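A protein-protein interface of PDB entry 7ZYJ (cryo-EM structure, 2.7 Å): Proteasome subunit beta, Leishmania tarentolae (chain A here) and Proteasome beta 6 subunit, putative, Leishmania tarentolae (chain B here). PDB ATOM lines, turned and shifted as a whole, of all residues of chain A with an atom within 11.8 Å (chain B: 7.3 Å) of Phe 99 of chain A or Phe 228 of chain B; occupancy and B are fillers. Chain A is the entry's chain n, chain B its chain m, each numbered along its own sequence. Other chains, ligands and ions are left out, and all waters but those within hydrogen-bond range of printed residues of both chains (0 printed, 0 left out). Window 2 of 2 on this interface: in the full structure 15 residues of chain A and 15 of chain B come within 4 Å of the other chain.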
ATOM      1  N   ASP A  55      13.745  33.556 -33.309  1.00  0.00           N
ATOM      2  CA  ASP A  55      13.133  32.544 -32.458  1.00  0.00           C
ATOM      3  C   ASP A  55      12.012  31.821 -33.192  1.00  0.00           C
ATOM      4  O   ASP A  55      11.881  30.597 -33.089  1.00  0.00           O
ATOM      5  CB  ASP A  55      12.609  33.184 -31.173  1.00  0.00           C
ATOM      6  CG  ASP A  55      13.718  33.751 -30.308  1.00  0.00           C
ATOM      7  OD1 ASP A  55      14.900  33.563 -30.656  1.00  0.00           O
ATOM      8  OD2 ASP A  55      13.407  34.386 -29.279  1.00  0.00           O
ATOM      9  N   ARG A  90       4.417  22.813 -25.704  1.00  0.00           N
ATOM     10  CA  ARG A  90       5.345  22.170 -24.779  1.00  0.00           C
ATOM     11  C   ARG A  90       6.775  22.621 -25.036  1.00  0.00           C
ATOM     12  O   ARG A  90       7.536  22.860 -24.091  1.00  0.00           O
ATOM     13  CB  ARG A  90       5.236  20.650 -24.884  1.00  0.00           C
ATOM     14  CG  ARG A  90       3.876  20.090 -24.517  1.00  0.00           C
ATOM     15  CD  ARG A  90       3.486  20.426 -23.092  1.00  0.00           C
ATOM     16  NE  ARG A  90       2.256  19.747 -22.707  1.00  0.00           N
ATOM     17  CZ  ARG A  90       1.449  20.145 -21.734  1.00  0.00           C
ATOM     18  NH1 ARG A  90       1.718  21.218 -21.010  1.00  0.00           N
ATOM     19  NH2 ARG A  90       0.343  19.451 -21.483  1.00  0.00           N
ATOM     20  N   SER A  91       7.158  22.754 -26.308  1.00  0.00           N
ATOM     21  CA  SER A  91       8.501  23.223 -26.629  1.00  0.00           C
ATOM     22  C   SER A  91       8.718  24.653 -26.150  1.00  0.00           C
ATOM     23  O   SER A  91       9.772  24.974 -25.587  1.00  0.00           O
ATOM     24  CB  SER A  91       8.746  23.117 -28.133  1.00  0.00           C
ATOM     25  OG  SER A  91       8.683  21.768 -28.561  1.00  0.00           O
ATOM     26  N   ILE A  92       7.726  25.522 -26.351  1.00  0.00           N
ATOM     27  CA  ILE A  92       7.851  26.908 -25.910  1.00  0.00           C
ATOM     28  C   ILE A  92       7.974  26.975 -24.393  1.00  0.00           C
ATOM     29  O   ILE A  92       8.815  27.704 -23.851  1.00  0.00           O
ATOM     30  CB  ILE A  92       6.661  27.740 -26.421  1.00  0.00           C
ATOM     31  CG1 ILE A  92       6.853  28.089 -27.897  1.00  0.00           C
ATOM     32  CG2 ILE A  92       6.488  29.002 -25.593  1.00  0.00           C
ATOM     33  CD1 ILE A  92       5.591  28.545 -28.582  1.00  0.00           C
ATOM     34  N   TYR A  93       7.143  26.207 -23.684  1.00  0.00           N
ATOM     35  CA  TYR A  93       7.204  26.207 -22.228  1.00  0.00           C
ATOM     36  C   TYR A  93       8.539  25.666 -21.732  1.00  0.00           C
ATOM     37  O   TYR A  93       9.102  26.180 -20.759  1.00  0.00           O
ATOM     38  CB  TYR A  93       6.044  25.395 -21.654  1.00  0.00           C
ATOM     39  CG  TYR A  93       5.989  25.404 -20.145  1.00  0.00           C
ATOM     40  CD1 TYR A  93       5.584  26.538 -19.455  1.00  0.00           C
ATOM     41  CD2 TYR A  93       6.341  24.282 -19.411  1.00  0.00           C
ATOM     42  CE1 TYR A  93       5.532  26.554 -18.076  1.00  0.00           C
ATOM     43  CE2 TYR A  93       6.291  24.290 -18.032  1.00  0.00           C
ATOM     44  CZ  TYR A  93       5.887  25.428 -17.371  1.00  0.00           C
ATOM     45  OH  TYR A  93       5.836  25.439 -15.996  1.00  0.00           O
ATOM     46  N   GLN A  94       9.061  24.624 -22.386  1.00  0.00           N
ATOM     47  CA  GLN A  94      10.363  24.090 -22.007  1.00  0.00           C
ATOM     48  C   GLN A  94      11.463  25.119 -22.229  1.00  0.00           C
ATOM     49  O   GLN A  94      12.394  25.224 -21.422  1.00  0.00           O
ATOM     50  CB  GLN A  94      10.653  22.810 -22.792  1.00  0.00           C
ATOM     51  CG  GLN A  94      11.989  22.171 -22.458  1.00  0.00           C
ATOM     52  CD  GLN A  94      12.164  21.941 -20.970  1.00  0.00           C
ATOM     53  OE1 GLN A  94      13.027  22.542 -20.334  1.00  0.00           O
ATOM     54  NE2 GLN A  94      11.338  21.068 -20.408  1.00  0.00           N
ATOM     55  N   LYS A  95      11.378  25.885 -23.321  1.00  0.00           N
ATOM     56  CA  LYS A  95      12.312  26.989 -23.515  1.00  0.00           C
ATOM     57  C   LYS A  95      12.193  28.022 -22.403  1.00  0.00           C
ATOM     58  O   LYS A  95      13.206  28.559 -21.946  1.00  0.00           O
ATOM     59  CB  LYS A  95      12.083  27.657 -24.871  1.00  0.00           C
ATOM     60  CG  LYS A  95      12.291  26.759 -26.076  1.00  0.00           C
ATOM     61  CD  LYS A  95      13.719  26.255 -26.155  1.00  0.00           C
ATOM     62  CE  LYS A  95      14.682  27.394 -26.437  1.00  0.00           C
ATOM     63  NZ  LYS A  95      14.445  28.000 -27.774  1.00  0.00           N
ATOM     64  N   ARG A  96      10.966  28.318 -21.965  1.00  0.00           N
ATOM     65  CA  ARG A  96      10.778  29.289 -20.892  1.00  0.00           C
ATOM     66  C   ARG A  96      11.390  28.802 -19.584  1.00  0.00           C
ATOM     67  O   ARG A  96      12.021  29.581 -18.861  1.00  0.00           O
ATOM     68  CB  ARG A  96       9.288  29.587 -20.717  1.00  0.00           C
ATOM     69  CG  ARG A  96       8.930  30.309 -19.429  1.00  0.00           C
ATOM     70  CD  ARG A  96       8.317  29.368 -18.405  1.00  0.00           C
ATOM     71  NE  ARG A  96       7.908  30.075 -17.197  1.00  0.00           N
ATOM     72  CZ  ARG A  96       7.731  29.499 -16.016  1.00  0.00           C
ATOM     73  NH1 ARG A  96       7.930  28.203 -15.842  1.00  0.00           N
ATOM     74  NH2 ARG A  96       7.347  30.243 -14.984  1.00  0.00           N
ATOM     75  N   CYS A  97      11.220  27.517 -19.262  1.00  0.00           N
ATOM     76  CA  CYS A  97      11.745  26.987 -18.009  1.00  0.00           C
ATOM     77  C   CYS A  97      13.266  26.926 -17.993  1.00  0.00           C
ATOM     78  O   CYS A  97      13.857  26.863 -16.910  1.00  0.00           O
ATOM     79  CB  CYS A  97      11.170  25.597 -17.743  1.00  0.00           C
ATOM     80  SG  CYS A  97       9.397  25.588 -17.421  1.00  0.00           S
ATOM     81  N   ASP A  98      13.908  26.946 -19.156  1.00  0.00           N
ATOM     82  CA  ASP A  98      15.360  26.962 -19.245  1.00  0.00           C
ATOM     83  C   ASP A  98      15.930  28.372 -19.246  1.00  0.00           C
ATOM     84  O   ASP A  98      17.143  28.534 -19.423  1.00  0.00           O
ATOM     85  CB  ASP A  98      15.820  26.222 -20.504  1.00  0.00           C
ATOM     86  CG  ASP A  98      15.505  24.741 -20.457  1.00  0.00           C
ATOM     87  OD1 ASP A  98      15.308  24.209 -19.345  1.00  0.00           O
ATOM     88  OD2 ASP A  98      15.456  24.108 -21.532  1.00  0.00           O
ATOM     89  N   PHE A  99      15.085  29.389 -19.065  1.00  0.00           N
ATOM     90  CA  PHE A  99      15.488  30.793 -19.110  1.00  0.00           C
ATOM     91  C   PHE A  99      16.103  31.162 -20.456  1.00  0.00           C
ATOM     92  O   PHE A  99      16.958  32.045 -20.543  1.00  0.00           O
ATOM     93  CB  PHE A  99      16.443  31.143 -17.963  1.00  0.00           C
ATOM     94  CG  PHE A  99      15.754  31.343 -16.643  1.00  0.00           C
ATOM     95  CD1 PHE A  99      15.059  30.306 -16.043  1.00  0.00           C
ATOM     96  CD2 PHE A  99      15.790  32.574 -16.010  1.00  0.00           C
ATOM     97  CE1 PHE A  99      14.421  30.490 -14.832  1.00  0.00           C
ATOM     98  CE2 PHE A  99      15.154  32.763 -14.798  1.00  0.00           C
ATOM     99  CZ  PHE A  99      14.468  31.720 -14.210  1.00  0.00           C
ATOM    100  N   ASP A 100      15.665  30.483 -21.514  1.00  0.00           N
ATOM    101  CA  ASP A 100      16.020  30.821 -22.891  1.00  0.00           C
ATOM    102  C   ASP A 100      14.738  30.847 -23.713  1.00  0.00           C
ATOM    103  O   ASP A 100      14.527  30.004 -24.592  1.00  0.00           O
ATOM    104  CB  ASP A 100      17.029  29.824 -23.462  1.00  0.00           C
ATOM    105  CG  ASP A 100      17.699  30.329 -24.722  1.00  0.00           C
ATOM    106  OD1 ASP A 100      17.973  31.544 -24.803  1.00  0.00           O
ATOM    107  OD2 ASP A 100      17.951  29.511 -25.631  1.00  0.00           O
ATOM    108  N   PRO A 101      13.857  31.807 -23.449  1.00  0.00           N
ATOM    109  CA  PRO A 101      12.515  31.760 -24.035  1.00  0.00           C
ATOM    110  C   PRO A 101      12.521  32.036 -25.530  1.00  0.00           C
ATOM    111  O   PRO A 101      13.425  32.669 -26.079  1.00  0.00           O
ATOM    112  CB  PRO A 101      11.762  32.857 -23.279  1.00  0.00           C
ATOM    113  CG  PRO A 101      12.824  33.827 -22.900  1.00  0.00           C
ATOM    114  CD  PRO A 101      14.052  33.008 -22.617  1.00  0.00           C
ATOM    115  N   CYS A 102      11.476  31.537 -26.186  1.00  0.00           N
ATOM    116  CA  CYS A 102      11.185  31.857 -27.580  1.00  0.00           C
ATOM    117  C   CYS A 102      10.304  33.100 -27.580  1.00  0.00           C
ATOM    118  O   CYS A 102       9.080  33.006 -27.478  1.00  0.00           O
ATOM    119  CB  CYS A 102      10.506  30.680 -28.270  1.00  0.00           C
ATOM    120  SG  CYS A 102       9.914  31.011 -29.942  1.00  0.00           S
ATOM    121  N   LEU A 103      10.929  34.271 -27.708  1.00  0.00           N
ATOM    122  CA  LEU A 103      10.249  35.552 -27.506  1.00  0.00           C
ATOM    123  C   LEU A 103       9.326  35.854 -28.686  1.00  0.00           C
ATOM    124  O   LEU A 103       9.545  36.770 -29.482  1.00  0.00           O
ATOM    125  CB  LEU A 103      11.270  36.662 -27.299  1.00  0.00           C
ATOM    126  CG  LEU A 103      12.114  36.568 -26.030  1.00  0.00           C
ATOM    127  CD1 LEU A 103      13.252  37.574 -26.070  1.00  0.00           C
ATOM    128  CD2 LEU A 103      11.250  36.780 -24.802  1.00  0.00           C
ATOM    129  N   ASP A 123       5.077  33.663 -25.415  1.00  0.00           N
ATOM    130  CA  ASP A 123       6.487  33.333 -25.271  1.00  0.00           C
ATOM    131  C   ASP A 123       6.807  32.676 -23.939  1.00  0.00           C
ATOM    132  O   ASP A 123       7.920  32.166 -23.768  1.00  0.00           O
ATOM    133  CB  ASP A 123       7.337  34.595 -25.424  1.00  0.00           C
ATOM    134  CG  ASP A 123       6.888  35.712 -24.506  1.00  0.00           C
ATOM    135  OD1 ASP A 123       5.684  36.044 -24.517  1.00  0.00           O
ATOM    136  OD2 ASP A 123       7.739  36.259 -23.774  1.00  0.00           O
ATOM    137  N   VAL A 124       5.869  32.678 -22.991  1.00  0.00           N
ATOM    138  CA  VAL A 124       6.135  32.152 -21.659  1.00  0.00           C
ATOM    139  C   VAL A 124       5.371  30.859 -21.396  1.00  0.00           C
ATOM    140  O   VAL A 124       5.571  30.231 -20.343  1.00  0.00           O
ATOM    141  CB  VAL A 124       5.808  33.220 -20.588  1.00  0.00           C
ATOM    142  CG1 VAL A 124       4.313  33.535 -20.560  1.00  0.00           C
ATOM    143  CG2 VAL A 124       6.385  32.871 -19.223  1.00  0.00           C
ATOM    144  N   GLY A 125       4.528  30.422 -22.331  1.00  0.00           N
ATOM    145  CA  GLY A 125       3.832  29.154 -22.220  1.00  0.00           C
ATOM    146  C   GLY A 125       2.326  29.245 -22.124  1.00  0.00           C
ATOM    147  O   GLY A 125       1.669  28.200 -22.063  1.00  0.00           O
ATOM    148  N   TRP B 126      12.516  40.695 -19.606  1.00  0.00           N
ATOM    149  CA  TRP B 126      11.621  39.546 -19.687  1.00  0.00           C
ATOM    150  C   TRP B 126      11.536  38.806 -18.358  1.00  0.00           C
ATOM    151  O   TRP B 126      12.554  38.498 -17.741  1.00  0.00           O
ATOM    152  CB  TRP B 126      12.078  38.584 -20.787  1.00  0.00           C
ATOM    153  CG  TRP B 126      11.237  37.348 -20.881  1.00  0.00           C
ATOM    154  CD1 TRP B 126      10.054  37.210 -21.546  1.00  0.00           C
ATOM    155  CD2 TRP B 126      11.515  36.073 -20.290  1.00  0.00           C
ATOM    156  NE1 TRP B 126       9.579  35.929 -21.405  1.00  0.00           N
ATOM    157  CE2 TRP B 126      10.458  35.211 -20.639  1.00  0.00           C
ATOM    158  CE3 TRP B 126      12.556  35.576 -19.499  1.00  0.00           C
ATOM    159  CZ2 TRP B 126      10.410  33.882 -20.225  1.00  0.00           C
ATOM    160  CZ3 TRP B 126      12.507  34.257 -19.090  1.00  0.00           C
ATOM    161  CH2 TRP B 126      11.442  33.424 -19.455  1.00  0.00           C
ATOM    162  N   SER B 127      10.310  38.524 -17.927  1.00  0.00           N
ATOM    163  CA  SER B 127      10.076  37.761 -16.715  1.00  0.00           C
ATOM    164  C   SER B 127       9.407  36.433 -17.046  1.00  0.00           C
ATOM    165  O   SER B 127       8.523  36.384 -17.909  1.00  0.00           O
ATOM    166  CB  SER B 127       9.195  38.541 -15.732  1.00  0.00           C
ATOM    167  OG  SER B 127       8.982  37.802 -14.543  1.00  0.00           O
ATOM    168  N   PRO B 128       9.801  35.344 -16.385  1.00  0.00           N
ATOM    169  CA  PRO B 128       9.180  34.041 -16.642  1.00  0.00           C
ATOM    170  C   PRO B 128       7.818  33.849 -15.995  1.00  0.00           C
ATOM    171  O   PRO B 128       7.273  32.745 -16.069  1.00  0.00           O
ATOM    172  CB  PRO B 128      10.203  33.063 -16.047  1.00  0.00           C
ATOM    173  CG  PRO B 128      10.840  33.827 -14.946  1.00  0.00           C
ATOM    174  CD  PRO B 128      10.901  35.255 -15.409  1.00  0.00           C
ATOM    175  N   TYR B 129       7.255  34.879 -15.371  1.00  0.00           N
ATOM    176  CA  TYR B 129       5.999  34.770 -14.648  1.00  0.00           C
ATOM    177  C   TYR B 129       4.962  35.714 -15.239  1.00  0.00           C
ATOM    178  O   TYR B 129       5.291  36.731 -15.856  1.00  0.00           O
ATOM    179  CB  TYR B 129       6.186  35.074 -13.157  1.00  0.00           C
ATOM    180  CG  TYR B 129       6.933  34.003 -12.398  1.00  0.00           C
ATOM    181  CD1 TYR B 129       6.451  32.703 -12.341  1.00  0.00           C
ATOM    182  CD2 TYR B 129       8.118  34.292 -11.735  1.00  0.00           C
ATOM    183  CE1 TYR B 129       7.128  31.721 -11.647  1.00  0.00           C
ATOM    184  CE2 TYR B 129       8.803  33.314 -11.038  1.00  0.00           C
ATOM    185  CZ  TYR B 129       8.301  32.031 -10.998  1.00  0.00           C
ATOM    186  OH  TYR B 129       8.977  31.053 -10.306  1.00  0.00           O
ATOM    187  N   ASP B 185       1.860  27.551 -15.758  1.00  0.00           N
ATOM    188  CA  ASP B 185       2.322  26.853 -14.567  1.00  0.00           C
ATOM    189  C   ASP B 185       1.298  25.831 -14.095  1.00  0.00           C
ATOM    190  O   ASP B 185       1.663  24.711 -13.722  1.00  0.00           O
ATOM    191  CB  ASP B 185       2.637  27.856 -13.459  1.00  0.00           C
ATOM    192  CG  ASP B 185       4.057  28.371 -13.528  1.00  0.00           C
ATOM    193  OD1 ASP B 185       4.728  28.127 -14.552  1.00  0.00           O
ATOM    194  OD2 ASP B 185       4.507  29.015 -12.559  1.00  0.00           O
ATOM    195  N   LEU B 222       4.946  20.574  -4.815  1.00  0.00           N
ATOM    196  CA  LEU B 222       5.078  22.025  -4.785  1.00  0.00           C
ATOM    197  C   LEU B 222       6.335  22.442  -4.037  1.00  0.00           C
ATOM    198  O   LEU B 222       7.027  23.378  -4.451  1.00  0.00           O
ATOM    199  CB  LEU B 222       3.842  22.662  -4.155  1.00  0.00           C
ATOM    200  CG  LEU B 222       2.575  22.715  -5.009  1.00  0.00           C
ATOM    201  CD1 LEU B 222       1.433  23.341  -4.230  1.00  0.00           C
ATOM    202  CD2 LEU B 222       2.831  23.478  -6.295  1.00  0.00           C
ATOM    203  N   HIS B 224       9.049  20.658  -3.761  1.00  0.00           N
ATOM    204  CA  HIS B 224      10.242  20.238  -4.490  1.00  0.00           C
ATOM    205  C   HIS B 224      10.743  21.334  -5.417  1.00  0.00           C
ATOM    206  O   HIS B 224      11.955  21.485  -5.604  1.00  0.00           O
ATOM    207  CB  HIS B 224       9.959  18.958  -5.275  1.00  0.00           C
ATOM    208  CG  HIS B 224       9.958  17.722  -4.432  1.00  0.00           C
ATOM    209  ND1 HIS B 224      10.442  17.703  -3.142  1.00  0.00           N
ATOM    210  CD2 HIS B 224       9.536  16.463  -4.694  1.00  0.00           C
ATOM    211  CE1 HIS B 224      10.317  16.485  -2.644  1.00  0.00           C
ATOM    212  NE2 HIS B 224       9.770  15.714  -3.567  1.00  0.00           N
ATOM    213  N   ARG B 225       9.833  22.105  -6.004  1.00  0.00           N
ATOM    214  CA  ARG B 225      10.196  23.282  -6.792  1.00  0.00           C
ATOM    215  C   ARG B 225      10.163  24.540  -5.922  1.00  0.00           C
ATOM    216  O   ARG B 225       9.514  25.530  -6.239  1.00  0.00           O
ATOM    217  CB  ARG B 225       9.261  23.414  -7.990  1.00  0.00           C
ATOM    218  CG  ARG B 225       9.597  22.506  -9.157  1.00  0.00           C
ATOM    219  CD  ARG B 225      10.473  23.227 -10.162  1.00  0.00           C
ATOM    220  NE  ARG B 225       9.883  24.496 -10.568  1.00  0.00           N
ATOM    221  CZ  ARG B 225       8.998  24.631 -11.546  1.00  0.00           C
ATOM    222  NH1 ARG B 225       8.588  23.593 -12.255  1.00  0.00           N
ATOM    223  NH2 ARG B 225       8.513  25.839 -11.820  1.00  0.00           N
ATOM    224  N   ARG B 226      10.876  24.487  -4.796  1.00  0.00           N
ATOM    225  CA  ARG B 226      10.815  25.602  -3.856  1.00  0.00           C
ATOM    226  C   ARG B 226      11.663  26.779  -4.323  1.00  0.00           C
ATOM    227  O   ARG B 226      11.338  27.931  -4.018  1.00  0.00           O
ATOM    228  CB  ARG B 226      11.251  25.142  -2.459  1.00  0.00           C
ATOM    229  CG  ARG B 226      11.084  26.174  -1.344  1.00  0.00           C
ATOM    230  CD  ARG B 226      12.314  27.035  -1.116  1.00  0.00           C
ATOM    231  NE  ARG B 226      12.153  27.893   0.053  1.00  0.00           N
ATOM    232  CZ  ARG B 226      12.989  28.865   0.390  1.00  0.00           C
ATOM    233  NH1 ARG B 226      14.063  29.135  -0.333  1.00  0.00           N
ATOM    234  NH2 ARG B 226      12.738  29.587   1.479  1.00  0.00           N
ATOM    235  N   PHE B 227      12.731  26.516  -5.075  1.00  0.00           N
ATOM    236  CA  PHE B 227      13.646  27.560  -5.512  1.00  0.00           C
ATOM    237  C   PHE B 227      13.269  28.164  -6.858  1.00  0.00           C
ATOM    238  O   PHE B 227      13.719  29.273  -7.167  1.00  0.00           O
ATOM    239  CB  PHE B 227      15.074  27.009  -5.575  1.00  0.00           C
ATOM    240  CG  PHE B 227      15.546  26.421  -4.277  1.00  0.00           C
ATOM    241  CD1 PHE B 227      15.599  27.197  -3.131  1.00  0.00           C
ATOM    242  CD2 PHE B 227      15.928  25.093  -4.198  1.00  0.00           C
ATOM    243  CE1 PHE B 227      16.029  26.662  -1.933  1.00  0.00           C
ATOM    244  CE2 PHE B 227      16.358  24.551  -3.002  1.00  0.00           C
ATOM    245  CZ  PHE B 227      16.408  25.338  -1.868  1.00  0.00           C
ATOM    246  N   PHE B 228      12.466  27.470  -7.659  1.00  0.00           N
ATOM    247  CA  PHE B 228      11.853  28.029  -8.864  1.00  0.00           C
ATOM    248  C   PHE B 228      10.371  27.695  -8.781  1.00  0.00           C
ATOM    249  O   PHE B 228       9.879  26.808  -9.491  1.00  0.00           O
ATOM    250  CB  PHE B 228      12.497  27.477 -10.135  1.00  0.00           C
ATOM    251  CG  PHE B 228      11.923  28.048 -11.400  1.00  0.00           C
ATOM    252  CD1 PHE B 228      11.645  29.401 -11.499  1.00  0.00           C
ATOM    253  CD2 PHE B 228      11.668  27.236 -12.492  1.00  0.00           C
ATOM    254  CE1 PHE B 228      11.118  29.931 -12.661  1.00  0.00           C
ATOM    255  CE2 PHE B 228      11.142  27.761 -13.657  1.00  0.00           C
ATOM    256  CZ  PHE B 228      10.867  29.110 -13.741  1.00  0.00           C
ATOM    257  N   PRO B 229       9.633  28.378  -7.911  1.00  0.00           N
ATOM    258  CA  PRO B 229       8.264  27.953  -7.606  1.00  0.00           C
ATOM    259  C   PRO B 229       7.324  28.104  -8.791  1.00  0.00           C
ATOM    260  O   PRO B 229       7.491  28.965  -9.658  1.00  0.00           O
ATOM    261  CB  PRO B 229       7.850  28.877  -6.455  1.00  0.00           C
ATOM    262  CG  PRO B 229       8.747  30.057  -6.570  1.00  0.00           C
ATOM    263  CD  PRO B 229      10.040  29.554  -7.124  1.00  0.00           C
ATOM    264  N   TYR B 230       6.326  27.227  -8.818  1.00  0.00           N
ATOM    265  CA  TYR B 230       5.179  27.431  -9.686  1.00  0.00           C
ATOM    266  C   TYR B 230       4.431  28.678  -9.241  1.00  0.00           C
ATOM    267  O   TYR B 230       4.295  28.943  -8.043  1.00  0.00           O
ATOM    268  CB  TYR B 230       4.239  26.226  -9.631  1.00  0.00           C
ATOM    269  CG  TYR B 230       4.779  24.953 -10.237  1.00  0.00           C
ATOM    270  CD1 TYR B 230       4.765  24.752 -11.610  1.00  0.00           C
ATOM    271  CD2 TYR B 230       5.278  23.938  -9.431  1.00  0.00           C
ATOM    272  CE1 TYR B 230       5.247  23.582 -12.164  1.00  0.00           C
ATOM    273  CE2 TYR B 230       5.762  22.766  -9.976  1.00  0.00           C
ATOM    274  CZ  TYR B 230       5.744  22.593 -11.343  1.00  0.00           C
ATOM    275  OH  TYR B 230       6.225  21.428 -11.889  1.00  0.00           O
ATOM    276  N   TYR B 231       3.939  29.447 -10.203  1.00  0.00           N
ATOM    277  CA  TYR B 231       3.118  30.614  -9.887  1.00  0.00           C
ATOM    278  C   TYR B 231       1.645  30.215  -9.848  1.00  0.00           C
ATOM    279  O   TYR B 231       0.797  30.751 -10.560  1.00  0.00           O
ATOM    280  CB  TYR B 231       3.373  31.732 -10.893  1.00  0.00           C
ATOM    281  CG  TYR B 231       2.760  33.054 -10.492  1.00  0.00           C
ATOM    282  CD1 TYR B 231       2.503  33.345  -9.159  1.00  0.00           C
ATOM    283  CD2 TYR B 231       2.447  34.015 -11.443  1.00  0.00           C
ATOM    284  CE1 TYR B 231       1.947  34.550  -8.785  1.00  0.00           C
ATOM    285  CE2 TYR B 231       1.891  35.224 -11.078  1.00  0.00           C
ATOM    286  CZ  TYR B 231       1.643  35.486  -9.748  1.00  0.00           C
ATOM    287  OH  TYR B 231       1.088  36.690  -9.377  1.00  0.00           O
ATOM    288  N   VAL B 253       4.519  27.581  -2.407  1.00  0.00           N
ATOM    289  CA  VAL B 253       5.559  26.600  -2.119  1.00  0.00           C
ATOM    290  C   VAL B 253       5.007  25.357  -1.428  1.00  0.00           C
ATOM    291  O   VAL B 253       5.783  24.515  -0.968  1.00  0.00           O
ATOM    292  CB  VAL B 253       6.694  27.225  -1.295  1.00  0.00           C
ATOM    293  CG1 VAL B 253       7.554  28.114  -2.176  1.00  0.00           C
ATOM    294  CG2 VAL B 253       6.127  28.020  -0.134  1.00  0.00           C
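Among the printed residues, pairs that only touch across the chains: Arg 96 of chain A with Trp 126 of chain B (3.9 Å), Arg 96 of chain A with Tyr 129 of chain B (3.7 Å), Arg 96 of chain A with Phe 228 of chain B (3.7 Å), Phe 99 of chain A with Phe 228 of chain B (3.97 Å), Pro 101 of chain A with Trp 126 of chain B (3.5 Å), Leu 103 of chain A with Trp 126 of chain B (3.5 Å) and Val 124 of chain A with Pro 128 of chain B (3.3 Å).
Asp 55 of chain A touches none of the printed residues of chain B. Of the printed residues of chain B, Tyr 93 of chain A touches Asp 185. Of the printed residues of chain B, Pro 101 of chain A touches Trp 126 (3.5 Å). Of the printed residues of chain B, Asp 123 of chain A touches Trp 126 (3.0 Å). Printed residues of chain A within 4 Å of Asp 185 of chain B: Tyr 93 and Arg 96. No residue of chain A comes within 4 Å of Arg 225 of chain B. No residue of chain A comes within 4 Å of Phe 227 of chain B. No residue of chain A comes within 4 Å of Pro 229 of chain B. No residue of chain A comes within 4 Å of Tyr 230 of chain B. Tyr 231 of chain B touches none of the printed residues of chain A. The nearest residue of chain B that does not touch Phe 99 of chain A is Pro 128 of chain B (4.3 Å). The nearest residue of chain A that does not touch Phe 228 of chain B is Cys 97 of chain A (4.3 Å).
The side-chain hydroxyl (OG) of Ser 127 of chain B sits close to the backbone NH (N) of Tyr 129 of chain B (3.5 Å). The side-chain hydroxyl of Tyr 129 of chain B sits at hydrogen-bond distance from the backbone carbonyl oxygen of Pro 229 of chain B, at 2.6 Å. The backbone NH (N) of Tyr 231 of chain B is in hydrogen-bond range of the side-chain carboxylate (OD2) of Asp 185 of chain B, 2.5 Å away. The side-chain carboxylate of Asp 55 of chain A sits at hydrogen-bond distance from the backbone NH of Leu 103 of chain A, 2.9 Å away. The side-chain sulfur (SG) of Cys 97 of chain A is in hydrogen-bond range of the backbone carbonyl oxygen (O) of Tyr 93 of chain A, 3.4 Å away. The side-chain sulfur (SG) of Cys 97 of chain A sits at hydrogen-bond distance from the guanidinium group (NH1) of Arg 96 of chain A, at 3.4 Å.
Printed residues of chain A that touch a printed residue of chain B: Tyr 93, Arg 96, Phe 99, Pro 101, Leu 103, Asp 123 and Val 124. Printed residues of chain B that touch a printed residue of chain A: Trp 126, Pro 128, Tyr 129, Asp 185 and Phe 228.
NE1 of Trp 126 of chain B sits at hydrogen-bond distance from OD2 of Asp 123 of chain A, 3.0 Å away. O of Pro 128 of chain B lies within hydrogen-bond range of NH2 of Arg 96 of chain A. OH of Tyr 93 of chain A lies within hydrogen-bond range of OD1 of Asp 185 of chain B. The guanidinium group (NH2) of Arg 96 of chain A is in salt-bridge range of the side-chain carboxylate (OD1) of Asp 185 of chain B, 3.4 Å away.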
